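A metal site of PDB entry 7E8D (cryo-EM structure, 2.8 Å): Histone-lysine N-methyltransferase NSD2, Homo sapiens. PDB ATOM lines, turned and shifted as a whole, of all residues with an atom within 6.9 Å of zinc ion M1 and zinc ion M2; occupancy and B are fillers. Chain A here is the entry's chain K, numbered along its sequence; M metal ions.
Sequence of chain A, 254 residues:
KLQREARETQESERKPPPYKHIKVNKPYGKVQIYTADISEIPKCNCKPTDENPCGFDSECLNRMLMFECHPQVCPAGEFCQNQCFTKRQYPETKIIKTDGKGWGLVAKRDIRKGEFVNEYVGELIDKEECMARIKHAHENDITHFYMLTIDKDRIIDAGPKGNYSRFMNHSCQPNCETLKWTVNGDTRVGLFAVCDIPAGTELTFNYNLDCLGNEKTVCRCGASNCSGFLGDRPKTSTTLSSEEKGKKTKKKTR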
ATOM      1  N   LYS A  43      -3.732  13.867   6.090  1.00  0.00           N
ATOM      2  CA  LYS A  43      -4.780  14.535   5.351  1.00  0.00           C
ATOM      3  C   LYS A  43      -5.767  13.499   4.858  1.00  0.00           C
ATOM      4  O   LYS A  43      -5.355  12.467   4.308  1.00  0.00           O
ATOM      5  CB  LYS A  43      -4.188  15.316   4.176  1.00  0.00           C
ATOM      6  CG  LYS A  43      -5.204  16.079   3.364  1.00  0.00           C
ATOM      7  CD  LYS A  43      -5.021  15.832   1.872  1.00  0.00           C
ATOM      8  CE  LYS A  43      -3.606  16.163   1.445  1.00  0.00           C
ATOM      9  NZ  LYS A  43      -3.404  15.790   0.021  1.00  0.00           N
ATOM     10  N   CYS A  44      -7.048  13.758   5.039  1.00  0.00           N
ATOM     11  CA  CYS A  44      -8.071  12.777   4.690  1.00  0.00           C
ATOM     12  C   CYS A  44      -8.437  12.900   3.213  1.00  0.00           C
ATOM     13  O   CYS A  44      -7.760  13.564   2.425  1.00  0.00           O
ATOM     14  CB  CYS A  44      -9.292  12.947   5.581  1.00  0.00           C
ATOM     15  SG  CYS A  44     -10.081  14.545   5.470  1.00  0.00           S
ATOM     16  N   ASN A  45      -9.526  12.236   2.829  1.00  0.00           N
ATOM     17  CA  ASN A  45     -10.054  12.296   1.474  1.00  0.00           C
ATOM     18  C   ASN A  45     -11.411  12.967   1.420  1.00  0.00           C
ATOM     19  O   ASN A  45     -12.070  12.923   0.387  1.00  0.00           O
ATOM     20  CB  ASN A  45     -10.145  10.896   0.880  1.00  0.00           C
ATOM     21  CG  ASN A  45      -8.787  10.305   0.576  1.00  0.00           C
ATOM     22  OD1 ASN A  45      -7.891  11.005   0.136  1.00  0.00           O
ATOM     23  ND2 ASN A  45      -8.647   9.015   0.820  1.00  0.00           N
ATOM     24  N   CYS A  46     -11.843  13.586   2.521  1.00  0.00           N
ATOM     25  CA  CYS A  46     -13.130  14.252   2.528  1.00  0.00           C
ATOM     26  C   CYS A  46     -13.084  15.476   1.615  1.00  0.00           C
ATOM     27  O   CYS A  46     -12.034  16.068   1.366  1.00  0.00           O
ATOM     28  CB  CYS A  46     -13.504  14.665   3.947  1.00  0.00           C
ATOM     29  SG  CYS A  46     -13.715  13.278   5.076  1.00  0.00           S
ATOM     30  N   LYS A  47     -14.260  15.841   1.097  1.00  0.00           N
ATOM     31  CA  LYS A  47     -14.330  16.946   0.170  1.00  0.00           C
ATOM     32  C   LYS A  47     -15.197  18.065   0.732  1.00  0.00           C
ATOM     33  O   LYS A  47     -16.163  17.799   1.450  1.00  0.00           O
ATOM     34  CB  LYS A  47     -14.892  16.489  -1.180  1.00  0.00           C
ATOM     35  CG  LYS A  47     -14.022  15.467  -1.872  1.00  0.00           C
ATOM     36  CD  LYS A  47     -14.649  15.014  -3.181  1.00  0.00           C
ATOM     37  CE  LYS A  47     -15.981  14.343  -2.935  1.00  0.00           C
ATOM     38  NZ  LYS A  47     -15.816  13.212  -2.006  1.00  0.00           N
ATOM     39  N   ASP A  50     -19.027  17.792   0.503  1.00  0.00           N
ATOM     40  CA  ASP A  50     -19.690  16.623   1.035  1.00  0.00           C
ATOM     41  C   ASP A  50     -20.853  17.027   1.929  1.00  0.00           C
ATOM     42  O   ASP A  50     -21.057  18.199   2.254  1.00  0.00           O
ATOM     43  CB  ASP A  50     -18.697  15.754   1.802  1.00  0.00           C
ATOM     44  CG  ASP A  50     -17.555  15.267   0.929  1.00  0.00           C
ATOM     45  OD1 ASP A  50     -17.742  15.217  -0.300  1.00  0.00           O
ATOM     46  OD2 ASP A  50     -16.476  14.940   1.471  1.00  0.00           O
ATOM     47  N   ASN A  52     -21.333  16.282   5.095  1.00  0.00           N
ATOM     48  CA  ASN A  52     -20.769  16.791   6.342  1.00  0.00           C
ATOM     49  C   ASN A  52     -19.284  16.511   6.315  1.00  0.00           C
ATOM     50  O   ASN A  52     -18.824  15.487   6.827  1.00  0.00           O
ATOM     51  CB  ASN A  52     -21.413  16.165   7.568  1.00  0.00           C
ATOM     52  CG  ASN A  52     -22.616  16.936   8.046  1.00  0.00           C
ATOM     53  OD1 ASN A  52     -22.496  18.055   8.530  1.00  0.00           O
ATOM     54  ND2 ASN A  52     -23.790  16.340   7.922  1.00  0.00           N
ATOM     55  N   PRO A  53     -18.488  17.412   5.736  1.00  0.00           N
ATOM     56  CA  PRO A  53     -17.070  17.125   5.535  1.00  0.00           C
ATOM     57  C   PRO A  53     -16.366  16.872   6.850  1.00  0.00           C
ATOM     58  O   PRO A  53     -16.395  17.705   7.764  1.00  0.00           O
ATOM     59  CB  PRO A  53     -16.551  18.405   4.857  1.00  0.00           C
ATOM     60  CG  PRO A  53     -17.754  19.043   4.288  1.00  0.00           C
ATOM     61  CD  PRO A  53     -18.868  18.735   5.229  1.00  0.00           C
ATOM     62  N   CYS A  54     -15.737  15.708   6.952  1.00  0.00           N
ATOM     63  CA  CYS A  54     -15.049  15.284   8.166  1.00  0.00           C
ATOM     64  C   CYS A  54     -15.992  15.271   9.361  1.00  0.00           C
ATOM     65  O   CYS A  54     -15.575  15.461  10.492  1.00  0.00           O
ATOM     66  CB  CYS A  54     -13.841  16.163   8.433  1.00  0.00           C
ATOM     67  SG  CYS A  54     -12.813  16.397   6.999  1.00  0.00           S
ATOM     68  N   GLY A  55     -17.273  15.048   9.096  1.00  0.00           N
ATOM     69  CA  GLY A  55     -18.261  15.079  10.144  1.00  0.00           C
ATOM     70  C   GLY A  55     -18.154  13.892  11.072  1.00  0.00           C
ATOM     71  O   GLY A  55     -17.389  12.955  10.849  1.00  0.00           O
ATOM     72  N   SER A  58     -19.612  10.704   9.298  1.00  0.00           N
ATOM     73  CA  SER A  58     -19.107  10.419   7.967  1.00  0.00           C
ATOM     74  C   SER A  58     -17.966   9.409   8.050  1.00  0.00           C
ATOM     75  O   SER A  58     -17.685   8.835   9.100  1.00  0.00           O
ATOM     76  CB  SER A  58     -18.677  11.718   7.291  1.00  0.00           C
ATOM     77  OG  SER A  58     -17.820  12.462   8.140  1.00  0.00           O
ATOM     78  N   GLU A  59     -17.295   9.181   6.921  1.00  0.00           N
ATOM     79  CA  GLU A  59     -16.177   8.246   6.850  1.00  0.00           C
ATOM     80  C   GLU A  59     -14.833   8.956   6.828  1.00  0.00           C
ATOM     81  O   GLU A  59     -13.932   8.547   6.093  1.00  0.00           O
ATOM     82  CB  GLU A  59     -16.313   7.344   5.622  1.00  0.00           C
ATOM     83  CG  GLU A  59     -17.238   6.157   5.804  1.00  0.00           C
ATOM     84  CD  GLU A  59     -18.685   6.572   5.880  1.00  0.00           C
ATOM     85  OE1 GLU A  59     -19.018   7.659   5.370  1.00  0.00           O
ATOM     86  OE2 GLU A  59     -19.490   5.813   6.463  1.00  0.00           O
ATOM     87  N   CYS A  60     -14.677  10.027   7.603  1.00  0.00           N
ATOM     88  CA  CYS A  60     -13.410  10.749   7.603  1.00  0.00           C
ATOM     89  C   CYS A  60     -12.281   9.830   8.025  1.00  0.00           C
ATOM     90  O   CYS A  60     -12.346   9.186   9.065  1.00  0.00           O
ATOM     91  CB  CYS A  60     -13.482  11.955   8.520  1.00  0.00           C
ATOM     92  SG  CYS A  60     -12.009  12.989   8.456  1.00  0.00           S
ATOM     93  N   LEU A  61     -11.242   9.792   7.211  1.00  0.00           N
ATOM     94  CA  LEU A  61     -10.112   8.921   7.494  1.00  0.00           C
ATOM     95  C   LEU A  61      -9.253   9.448   8.632  1.00  0.00           C
ATOM     96  O   LEU A  61      -8.461   8.690   9.187  1.00  0.00           O
ATOM     97  CB  LEU A  61      -9.266   8.764   6.239  1.00  0.00           C
ATOM     98  CG  LEU A  61      -8.423   7.502   6.157  1.00  0.00           C
ATOM     99  CD1 LEU A  61      -9.213   6.324   6.648  1.00  0.00           C
ATOM    100  CD2 LEU A  61      -8.006   7.294   4.739  1.00  0.00           C
ATOM    101  N   ASN A  62      -9.385  10.717   8.985  1.00  0.00           N
ATOM    102  CA  ASN A  62      -8.709  11.214  10.175  1.00  0.00           C
ATOM    103  C   ASN A  62      -9.533  10.939  11.413  1.00  0.00           C
ATOM    104  O   ASN A  62      -8.987  10.612  12.480  1.00  0.00           O
ATOM    105  CB  ASN A  62      -8.430  12.701  10.051  1.00  0.00           C
ATOM    106  CG  ASN A  62      -7.245  12.996   9.183  1.00  0.00           C
ATOM    107  OD1 ASN A  62      -7.307  12.856   7.979  1.00  0.00           O
ATOM    108  ND2 ASN A  62      -6.150  13.413   9.792  1.00  0.00           N
ATOM    109  N   ARG A  63     -10.853  11.084  11.302  1.00  0.00           N
ATOM    110  CA  ARG A  63     -11.712  10.819  12.456  1.00  0.00           C
ATOM    111  C   ARG A  63     -11.699   9.350  12.815  1.00  0.00           C
ATOM    112  O   ARG A  63     -11.691   8.994  13.989  1.00  0.00           O
ATOM    113  CB  ARG A  63     -13.129  11.306  12.157  1.00  0.00           C
ATOM    114  CG  ARG A  63     -13.967  11.450  13.402  1.00  0.00           C
ATOM    115  CD  ARG A  63     -15.363  11.904  13.088  1.00  0.00           C
ATOM    116  NE  ARG A  63     -15.446  13.319  12.781  1.00  0.00           N
ATOM    117  CZ  ARG A  63     -15.679  14.267  13.693  1.00  0.00           C
ATOM    118  NH1 ARG A  63     -15.841  13.929  14.959  1.00  0.00           N
ATOM    119  NH2 ARG A  63     -15.746  15.532  13.325  1.00  0.00           N
ATOM    120  N   GLU A  68      -6.849  14.485  14.237  1.00  0.00           N
ATOM    121  CA  GLU A  68      -7.557  15.746  14.155  1.00  0.00           C
ATOM    122  C   GLU A  68      -7.164  16.438  12.862  1.00  0.00           C
ATOM    123  O   GLU A  68      -5.978  16.612  12.582  1.00  0.00           O
ATOM    124  CB  GLU A  68      -7.222  16.620  15.360  1.00  0.00           C
ATOM    125  CG  GLU A  68      -7.865  17.975  15.339  1.00  0.00           C
ATOM    126  CD  GLU A  68      -9.185  17.999  16.075  1.00  0.00           C
ATOM    127  OE1 GLU A  68      -9.900  16.985  16.062  1.00  0.00           O
ATOM    128  OE2 GLU A  68      -9.500  19.043  16.671  1.00  0.00           O
ATOM    129  N   CYS A  69      -8.160  16.831  12.067  1.00  0.00           N
ATOM    130  CA  CYS A  69      -7.861  17.536  10.832  1.00  0.00           C
ATOM    131  C   CYS A  69      -7.279  18.910  11.153  1.00  0.00           C
ATOM    132  O   CYS A  69      -7.404  19.416  12.270  1.00  0.00           O
ATOM    133  CB  CYS A  69      -9.116  17.680   9.976  1.00  0.00           C
ATOM    134  SG  CYS A  69      -9.524  16.237   9.001  1.00  0.00           S
ATOM    135  N   HIS A  70      -6.627  19.489  10.162  1.00  0.00           N
ATOM    136  CA  HIS A  70      -6.025  20.804  10.277  1.00  0.00           C
ATOM    137  C   HIS A  70      -6.603  21.672   9.175  1.00  0.00           C
ATOM    138  O   HIS A  70      -6.575  21.275   7.994  1.00  0.00           O
ATOM    139  CB  HIS A  70      -4.505  20.713  10.155  1.00  0.00           C
ATOM    140  CG  HIS A  70      -3.790  21.979  10.479  1.00  0.00           C
ATOM    141  ND1 HIS A  70      -4.063  23.174   9.843  1.00  0.00           N
ATOM    142  CD2 HIS A  70      -2.797  22.242  11.350  1.00  0.00           C
ATOM    143  CE1 HIS A  70      -3.268  24.107  10.319  1.00  0.00           C
ATOM    144  NE2 HIS A  70      -2.491  23.574  11.245  1.00  0.00           N
ATOM    145  N   PRO A  71      -7.149  22.844   9.503  1.00  0.00           N
ATOM    146  CA  PRO A  71      -7.836  23.645   8.473  1.00  0.00           C
ATOM    147  C   PRO A  71      -6.927  24.049   7.327  1.00  0.00           C
ATOM    148  O   PRO A  71      -7.410  24.209   6.193  1.00  0.00           O
ATOM    149  CB  PRO A  71      -8.339  24.861   9.260  1.00  0.00           C
ATOM    150  CG  PRO A  71      -7.395  24.960  10.415  1.00  0.00           C
ATOM    151  CD  PRO A  71      -7.058  23.557  10.793  1.00  0.00           C
ATOM    152  N   CYS A  74      -6.512  20.162   5.798  1.00  0.00           N
ATOM    153  CA  CYS A  74      -7.692  19.416   5.423  1.00  0.00           C
ATOM    154  C   CYS A  74      -8.213  19.919   4.081  1.00  0.00           C
ATOM    155  O   CYS A  74      -8.376  21.130   3.897  1.00  0.00           O
ATOM    156  CB  CYS A  74      -8.771  19.544   6.483  1.00  0.00           C
ATOM    157  SG  CYS A  74     -10.252  18.615   6.138  1.00  0.00           S
ATOM    158  N   PRO A  75      -8.480  19.031   3.121  1.00  0.00           N
ATOM    159  CA  PRO A  75      -9.038  19.488   1.844  1.00  0.00           C
ATOM    160  C   PRO A  75     -10.407  20.101   1.957  1.00  0.00           C
ATOM    161  O   PRO A  75     -10.820  20.814   1.047  1.00  0.00           O
ATOM    162  CB  PRO A  75      -9.062  18.201   1.006  1.00  0.00           C
ATOM    163  CG  PRO A  75      -9.158  17.122   2.005  1.00  0.00           C
ATOM    164  CD  PRO A  75      -8.349  17.571   3.170  1.00  0.00           C
ATOM    165  N   ALA A  76     -11.138  19.835   3.041  1.00  0.00           N
ATOM    166  CA  ALA A  76     -12.433  20.450   3.220  1.00  0.00           C
ATOM    167  C   ALA A  76     -12.335  21.909   3.630  1.00  0.00           C
ATOM    168  O   ALA A  76     -13.362  22.581   3.711  1.00  0.00           O
ATOM    169  CB  ALA A  76     -13.246  19.686   4.265  1.00  0.00           C
ATOM    170  N   GLY A  77     -11.129  22.403   3.897  1.00  0.00           N
ATOM    171  CA  GLY A  77     -10.943  23.799   4.224  1.00  0.00           C
ATOM    172  C   GLY A  77     -11.569  24.187   5.548  1.00  0.00           C
ATOM    173  O   GLY A  77     -11.059  23.821   6.607  1.00  0.00           O
ATOM    174  N   PHE A  79     -15.040  23.699   6.010  1.00  0.00           N
ATOM    175  CA  PHE A  79     -16.203  22.848   6.224  1.00  0.00           C
ATOM    176  C   PHE A  79     -15.876  21.619   7.067  1.00  0.00           C
ATOM    177  O   PHE A  79     -16.720  20.718   7.167  1.00  0.00           O
ATOM    178  CB  PHE A  79     -16.785  22.417   4.877  1.00  0.00           C
ATOM    179  CG  PHE A  79     -17.208  23.559   4.015  1.00  0.00           C
ATOM    180  CD1 PHE A  79     -16.297  24.207   3.193  1.00  0.00           C
ATOM    181  CD2 PHE A  79     -18.517  23.995   4.018  1.00  0.00           C
ATOM    182  CE1 PHE A  79     -16.699  25.254   2.392  1.00  0.00           C
ATOM    183  CE2 PHE A  79     -18.919  25.042   3.218  1.00  0.00           C
ATOM    184  CZ  PHE A  79     -18.001  25.675   2.411  1.00  0.00           C
ATOM    185  N   CYS A  80     -14.687  21.570   7.657  1.00  0.00           N
ATOM    186  CA  CYS A  80     -14.238  20.411   8.411  1.00  0.00           C
ATOM    187  C   CYS A  80     -14.815  20.475   9.818  1.00  0.00           C
ATOM    188  O   CYS A  80     -14.416  21.333  10.620  1.00  0.00           O
ATOM    189  CB  CYS A  80     -12.715  20.378   8.450  1.00  0.00           C
ATOM    190  SG  CYS A  80     -12.006  19.131   9.549  1.00  0.00           S
ATOM    191  N   GLN A  81     -15.735  19.569  10.134  1.00  0.00           N
ATOM    192  CA  GLN A  81     -16.256  19.437  11.487  1.00  0.00           C
ATOM    193  C   GLN A  81     -15.373  18.562  12.360  1.00  0.00           C
ATOM    194  O   GLN A  81     -15.859  18.008  13.350  1.00  0.00           O
ATOM    195  CB  GLN A  81     -17.678  18.880  11.465  1.00  0.00           C
ATOM    196  CG  GLN A  81     -18.676  19.733  10.705  1.00  0.00           C
ATOM    197  CD  GLN A  81     -18.816  19.297   9.275  1.00  0.00           C
ATOM    198  OE1 GLN A  81     -18.837  18.107   8.986  1.00  0.00           O
ATOM    199  NE2 GLN A  81     -18.913  20.270   8.370  1.00  0.00           N
ATOM    200  N   ASN A  82     -14.118  18.408  12.003  1.00  0.00           N
ATOM    201  CA  ASN A  82     -13.165  17.593  12.750  1.00  0.00           C
ATOM    202  C   ASN A  82     -12.038  18.446  13.314  1.00  0.00           C
ATOM    203  O   ASN A  82     -10.859  18.096  13.231  1.00  0.00           O
ATOM    204  CB  ASN A  82     -12.619  16.469  11.860  1.00  0.00           C
ATOM    205  CG  ASN A  82     -11.717  15.521  12.612  1.00  0.00           C
ATOM    206  OD1 ASN A  82     -11.702  15.497  13.843  1.00  0.00           O
ATOM    207  ND2 ASN A  82     -10.930  14.751  11.875  1.00  0.00           N
ATOM    208  N   GLN A  83     -12.375  19.590  13.886  1.00  0.00           N
ATOM    209  CA  GLN A  83     -11.409  20.415  14.578  1.00  0.00           C
ATOM    210  C   GLN A  83     -11.846  20.656  16.012  1.00  0.00           C
ATOM    211  O   GLN A  83     -11.612  21.723  16.582  1.00  0.00           O
ATOM    212  CB  GLN A  83     -11.176  21.729  13.837  1.00  0.00           C
ATOM    213  CG  GLN A  83     -10.621  21.524  12.456  1.00  0.00           C
ATOM    214  CD  GLN A  83     -10.632  22.790  11.645  1.00  0.00           C
ATOM    215  OE1 GLN A  83     -10.048  23.794  12.045  1.00  0.00           O
ATOM    216  NE2 GLN A  83     -11.291  22.748  10.502  1.00  0.00           N
HETATM  217 ZN    ZN M   1     -12.141  14.233   6.492  1.00  0.00          ZN
HETATM  218 ZN    ZN M   2     -11.128  17.595   8.026  1.00  0.00          ZN
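Within 4 Å of zinc ion M1: Cys 44, Cys 46, Cys 54 and Cys 60.
Along chain A the residues within 4 Å of zinc ion M1 span positions 44 to 60.
Zinc ion M2 is bound by SG of Cys 54, SG of Cys 69, SG of Cys 74 and SG of Cys 80.
Zinc ion M2 has four donor atoms within binding distance.
Four residues have an atom within 4 Å of zinc ion M2: Cys 54, Cys 69, Cys 74 and Cys 80.
Along chain A the residues within 4 Å of zinc ion M2 span positions 54 to 80.
The nearest printed residue that does not touch zinc ion M2 is Cys 44 (4.1 Å).
Zinc ion M1 is bound by the side-chain sulfur of Cys 44 (2.3 Å), the side-chain sulfur of Cys 54 (2.3 Å), the side-chain sulfur of Cys 46 (2.3 Å) and the side-chain sulfur of Cys 60 (2.3 Å).
Zinc ion M1 has four donor atoms within binding distance.
The guanidinium group (NH2) of Arg 63 sits at hydrogen-bond distance from the backbone carbonyl oxygen (O) of Cys 54, 2.8 Å away.
N of Cys 69 is in hydrogen-bond range of O of Asn 82 (3.2 Å).
The backbone NH (N) of Ala 76 sits close to the side-chain sulfur (SG) of Cys 74 (3.4 Å).
OD1 of Asn 62 lies within hydrogen-bond range of N of Cys 44 (3.1 Å).
The backbone NH of Asn 62 sits close to the side-chain sulfur of Cys 60 (3.5 Å).
SG of Cys 60 sits close to N of Arg 63, 3.6 Å away.
The side-chain sulfur (SG) of Cys 80 sits close to the backbone NH (N) of Asn 82.
The backbone carbonyl oxygen (O) of Cys 80 lies within hydrogen-bond range of the side-chain amide nitrogen (NE2) of Gln 83 (3.4 Å).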
